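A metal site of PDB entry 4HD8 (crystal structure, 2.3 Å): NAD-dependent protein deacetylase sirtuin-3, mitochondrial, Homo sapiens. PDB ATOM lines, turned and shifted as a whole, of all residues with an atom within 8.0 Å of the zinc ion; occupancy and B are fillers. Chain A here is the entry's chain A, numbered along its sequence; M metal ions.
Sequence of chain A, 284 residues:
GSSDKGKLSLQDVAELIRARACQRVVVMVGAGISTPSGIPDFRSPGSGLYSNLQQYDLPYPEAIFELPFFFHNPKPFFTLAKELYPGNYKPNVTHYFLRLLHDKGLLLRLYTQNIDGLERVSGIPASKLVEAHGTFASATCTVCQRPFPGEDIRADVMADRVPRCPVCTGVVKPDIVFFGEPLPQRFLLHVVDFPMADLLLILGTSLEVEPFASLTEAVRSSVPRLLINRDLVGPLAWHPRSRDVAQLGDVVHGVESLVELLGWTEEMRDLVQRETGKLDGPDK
The zinc ion is bound by SG of Cys 144, SG of Cys 165, SG of Cys 168 and SG of Cys 141.
Within 4 Å of the zinc ion: Cys 141, Cys 144, Cys 165 and Cys 168.
The side-chain sulfur (SG) of Cys 144 sits close to the guanidinium group (NH2) of Arg 146, 3.3 Å away. N of Cys 165 is in hydrogen-bond range of O of Gly 170, 2.7 Å away. The side-chain sulfur (SG) of Cys 165 lies close to the backbone NH (N) of Val 167. The side-chain sulfur (SG) of Cys 168 lies close to the backbone NH (N) of Gly 170. O of Arg 146 sits at hydrogen-bond distance from N of Cys 141, 2.8 Å away. N of Val 143 lies close to SG of Cys 141 (3.4 Å). The backbone carbonyl oxygen (O) of Cys 141 lies close to the side-chain amide nitrogen (NE2) of Gln 145 (3.3 Å).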
ATOM      1  N   THR A 140     -20.680  -8.153   9.114  1.00  0.00           N
ATOM      2  CA  THR A 140     -20.514  -8.093   7.664  1.00  0.00           C
ATOM      3  C   THR A 140     -20.424  -6.645   7.235  1.00  0.00           C
ATOM      4  O   THR A 140     -21.268  -5.847   7.657  1.00  0.00           O
ATOM      5  CB  THR A 140     -21.683  -8.837   6.944  1.00  0.00           C
ATOM      6  OG1 THR A 140     -21.555 -10.232   7.250  1.00  0.00           O
ATOM      7  CG2 THR A 140     -21.569  -8.714   5.429  1.00  0.00           C
ATOM      8  N   CYS A 141     -19.396  -6.290   6.440  1.00  0.00           N
ATOM      9  CA  CYS A 141     -19.352  -4.930   5.905  1.00  0.00           C
ATOM     10  C   CYS A 141     -20.628  -4.723   5.060  1.00  0.00           C
ATOM     11  O   CYS A 141     -20.933  -5.536   4.176  1.00  0.00           O
ATOM     12  CB  CYS A 141     -18.161  -4.725   4.985  1.00  0.00           C
ATOM     13  SG  CYS A 141     -18.142  -3.029   4.363  1.00  0.00           S
ATOM     14  N   THR A 142     -21.329  -3.616   5.309  1.00  0.00           N
ATOM     15  CA  THR A 142     -22.600  -3.287   4.674  1.00  0.00           C
ATOM     16  C   THR A 142     -22.398  -2.840   3.238  1.00  0.00           C
ATOM     17  O   THR A 142     -23.345  -2.755   2.523  1.00  0.00           O
ATOM     18  CB  THR A 142     -23.343  -2.156   5.443  1.00  0.00           C
ATOM     19  OG1 THR A 142     -22.432  -1.069   5.696  1.00  0.00           O
ATOM     20  CG2 THR A 142     -23.925  -2.692   6.797  1.00  0.00           C
ATOM     21  N   VAL A 143     -21.147  -2.543   2.851  1.00  0.00           N
ATOM     22  CA  VAL A 143     -20.812  -2.088   1.519  1.00  0.00           C
ATOM     23  C   VAL A 143     -20.136  -3.196   0.686  1.00  0.00           C
ATOM     24  O   VAL A 143     -20.650  -3.529  -0.362  1.00  0.00           O
ATOM     25  CB  VAL A 143     -19.972  -0.781   1.559  1.00  0.00           C
ATOM     26  CG1 VAL A 143     -19.716  -0.252   0.139  1.00  0.00           C
ATOM     27  CG2 VAL A 143     -20.702   0.296   2.361  1.00  0.00           C
ATOM     28  N   CYS A 144     -18.981  -3.754   1.096  1.00  0.00           N
ATOM     29  CA  CYS A 144     -18.298  -4.705   0.195  1.00  0.00           C
ATOM     30  C   CYS A 144     -18.623  -6.148   0.555  1.00  0.00           C
ATOM     31  O   CYS A 144     -18.085  -7.045  -0.053  1.00  0.00           O
ATOM     32  CB  CYS A 144     -16.784  -4.534   0.228  1.00  0.00           C
ATOM     33  SG  CYS A 144     -16.038  -4.969   1.833  1.00  0.00           S
ATOM     34  N   GLN A 145     -19.482  -6.381   1.549  1.00  0.00           N
ATOM     35  CA  GLN A 145     -19.862  -7.730   1.993  1.00  0.00           C
ATOM     36  C   GLN A 145     -18.726  -8.609   2.580  1.00  0.00           C
ATOM     37  O   GLN A 145     -18.886  -9.802   2.711  1.00  0.00           O
ATOM     38  CB  GLN A 145     -20.618  -8.461   0.874  1.00  0.00           C
ATOM     39  CG  GLN A 145     -21.801  -7.683   0.263  1.00  0.00           C
ATOM     40  CD  GLN A 145     -22.769  -7.148   1.297  1.00  0.00           C
ATOM     41  OE1 GLN A 145     -23.466  -7.927   1.983  1.00  0.00           O
ATOM     42  NE2 GLN A 145     -22.826  -5.831   1.444  1.00  0.00           N
ATOM     43  N   ARG A 146     -17.583  -8.043   2.925  1.00  0.00           N
ATOM     44  CA  ARG A 146     -16.576  -8.826   3.634  1.00  0.00           C
ATOM     45  C   ARG A 146     -17.124  -9.203   5.023  1.00  0.00           C
ATOM     46  O   ARG A 146     -17.608  -8.318   5.712  1.00  0.00           O
ATOM     47  CB  ARG A 146     -15.279  -8.051   3.835  1.00  0.00           C
ATOM     48  CG  ARG A 146     -14.417  -7.917   2.582  1.00  0.00           C
ATOM     49  CD  ARG A 146     -13.127  -7.128   2.939  1.00  0.00           C
ATOM     50  NE  ARG A 146     -12.106  -7.267   1.886  1.00  0.00           N
ATOM     51  CZ  ARG A 146     -12.148  -6.578   0.750  1.00  0.00           C
ATOM     52  NH1 ARG A 146     -11.233  -6.759  -0.190  1.00  0.00           N
ATOM     53  NH2 ARG A 146     -13.169  -5.741   0.512  1.00  0.00           N
ATOM     54  N   PRO A 147     -17.012 -10.517   5.424  1.00  0.00           N
ATOM     55  CA  PRO A 147     -17.300 -11.080   6.785  1.00  0.00           C
ATOM     56  C   PRO A 147     -16.097 -10.862   7.700  1.00  0.00           C
ATOM     57  O   PRO A 147     -14.985 -10.748   7.183  1.00  0.00           O
ATOM     58  CB  PRO A 147     -17.467 -12.605   6.539  1.00  0.00           C
ATOM     59  CG  PRO A 147     -16.619 -12.883   5.270  1.00  0.00           C
ATOM     60  CD  PRO A 147     -16.598 -11.589   4.451  1.00  0.00           C
ATOM     61  N   PHE A 148     -16.363 -10.778   9.014  1.00  0.00           N
ATOM     62  CA  PHE A 148     -15.430 -10.483  10.104  1.00  0.00           C
ATOM     63  C   PHE A 148     -15.965 -11.234  11.324  1.00  0.00           C
ATOM     64  O   PHE A 148     -17.167 -11.284  11.515  1.00  0.00           O
ATOM     65  CB  PHE A 148     -15.363  -8.985  10.490  1.00  0.00           C
ATOM     66  CG  PHE A 148     -14.832  -8.099   9.412  1.00  0.00           C
ATOM     67  CD1 PHE A 148     -13.442  -7.893   9.267  1.00  0.00           C
ATOM     68  CD2 PHE A 148     -15.699  -7.473   8.516  1.00  0.00           C
ATOM     69  CE1 PHE A 148     -12.935  -7.100   8.227  1.00  0.00           C
ATOM     70  CE2 PHE A 148     -15.201  -6.682   7.499  1.00  0.00           C
ATOM     71  CZ  PHE A 148     -13.826  -6.491   7.352  1.00  0.00           C
ATOM     72  N   ARG A 164     -15.767   0.303  11.241  1.00  0.00           N
ATOM     73  CA  ARG A 164     -15.633   0.655   9.830  1.00  0.00           C
ATOM     74  C   ARG A 164     -14.801  -0.426   9.081  1.00  0.00           C
ATOM     75  O   ARG A 164     -13.791  -0.878   9.599  1.00  0.00           O
ATOM     76  CB  ARG A 164     -14.911   2.013   9.717  1.00  0.00           C
ATOM     77  CG  ARG A 164     -15.663   3.209  10.263  1.00  0.00           C
ATOM     78  CD  ARG A 164     -16.490   3.753   9.129  1.00  0.00           C
ATOM     79  NE  ARG A 164     -17.520   4.657   9.536  1.00  0.00           N
ATOM     80  CZ  ARG A 164     -18.458   5.124   8.710  1.00  0.00           C
ATOM     81  NH1 ARG A 164     -18.457   4.767   7.423  1.00  0.00           N
ATOM     82  NH2 ARG A 164     -19.387   5.950   9.179  1.00  0.00           N
ATOM     83  N   CYS A 165     -15.186  -0.784   7.850  1.00  0.00           N
ATOM     84  CA  CYS A 165     -14.413  -1.779   7.056  1.00  0.00           C
ATOM     85  C   CYS A 165     -12.950  -1.316   6.831  1.00  0.00           C
ATOM     86  O   CYS A 165     -12.705  -0.166   6.380  1.00  0.00           O
ATOM     87  CB  CYS A 165     -15.134  -2.070   5.763  1.00  0.00           C
ATOM     88  SG  CYS A 165     -14.370  -3.344   4.718  1.00  0.00           S
ATOM     89  N   PRO A 166     -11.961  -2.189   7.181  1.00  0.00           N
ATOM     90  CA  PRO A 166     -10.548  -1.772   7.048  1.00  0.00           C
ATOM     91  C   PRO A 166     -10.155  -1.717   5.572  1.00  0.00           C
ATOM     92  O   PRO A 166      -9.079  -1.289   5.317  1.00  0.00           O
ATOM     93  CB  PRO A 166      -9.754  -2.871   7.823  1.00  0.00           C
ATOM     94  CG  PRO A 166     -10.654  -4.061   7.749  1.00  0.00           C
ATOM     95  CD  PRO A 166     -12.070  -3.505   7.829  1.00  0.00           C
ATOM     96  N   VAL A 167     -11.039  -2.106   4.645  1.00  0.00           N
ATOM     97  CA  VAL A 167     -10.792  -1.955   3.188  1.00  0.00           C
ATOM     98  C   VAL A 167     -11.617  -0.816   2.539  1.00  0.00           C
ATOM     99  O   VAL A 167     -11.040   0.116   1.982  1.00  0.00           O
ATOM    100  CB  VAL A 167     -11.003  -3.300   2.377  1.00  0.00           C
ATOM    101  CG1 VAL A 167     -10.836  -3.095   0.879  1.00  0.00           C
ATOM    102  CG2 VAL A 167     -10.073  -4.402   2.867  1.00  0.00           C
ATOM    103  N   CYS A 168     -12.963  -0.846   2.658  1.00  0.00           N
ATOM    104  CA  CYS A 168     -13.787   0.146   1.918  1.00  0.00           C
ATOM    105  C   CYS A 168     -14.299   1.285   2.804  1.00  0.00           C
ATOM    106  O   CYS A 168     -14.900   2.191   2.291  1.00  0.00           O
ATOM    107  CB  CYS A 168     -14.949  -0.517   1.148  1.00  0.00           C
ATOM    108  SG  CYS A 168     -16.311  -1.015   2.230  1.00  0.00           S
ATOM    109  N   THR A 169     -14.016   1.248   4.118  1.00  0.00           N
ATOM    110  CA  THR A 169     -14.606   2.199   5.108  1.00  0.00           C
ATOM    111  C   THR A 169     -16.133   2.026   5.377  1.00  0.00           C
ATOM    112  O   THR A 169     -16.648   2.699   6.249  1.00  0.00           O
ATOM    113  CB  THR A 169     -14.332   3.720   4.817  1.00  0.00           C
ATOM    114  OG1 THR A 169     -15.207   4.164   3.798  1.00  0.00           O
ATOM    115  CG2 THR A 169     -12.942   3.926   4.308  1.00  0.00           C
ATOM    116  N   GLY A 170     -16.827   1.156   4.659  1.00  0.00           N
ATOM    117  CA  GLY A 170     -18.253   0.898   4.923  1.00  0.00           C
ATOM    118  C   GLY A 170     -18.497   0.584   6.390  1.00  0.00           C
ATOM    119  O   GLY A 170     -17.623   0.017   7.089  1.00  0.00           O
ATOM    120  N   VAL A 171     -19.689   0.921   6.879  1.00  0.00           N
ATOM    121  CA  VAL A 171     -20.110   0.386   8.212  1.00  0.00           C
ATOM    122  C   VAL A 171     -20.175  -1.155   8.272  1.00  0.00           C
ATOM    123  O   VAL A 171     -20.724  -1.855   7.357  1.00  0.00           O
ATOM    124  CB  VAL A 171     -21.401   1.047   8.742  1.00  0.00           C
ATOM    125  CG1 VAL A 171     -21.711   0.544  10.159  1.00  0.00           C
ATOM    126  CG2 VAL A 171     -21.140   2.556   8.835  1.00  0.00           C
ATOM    127  N   VAL A 172     -19.591  -1.672   9.335  1.00  0.00           N
ATOM    128  CA  VAL A 172     -19.579  -3.089   9.529  1.00  0.00           C
ATOM    129  C   VAL A 172     -20.661  -3.439  10.541  1.00  0.00           C
ATOM    130  O   VAL A 172     -20.567  -3.067  11.717  1.00  0.00           O
ATOM    131  CB  VAL A 172     -18.209  -3.574  10.049  1.00  0.00           C
ATOM    132  CG1 VAL A 172     -18.301  -5.022  10.446  1.00  0.00           C
ATOM    133  CG2 VAL A 172     -17.129  -3.390   8.962  1.00  0.00           C
HETATM  134 ZN    ZN M   1     -16.083  -3.133   3.167  1.00  0.00          ZN
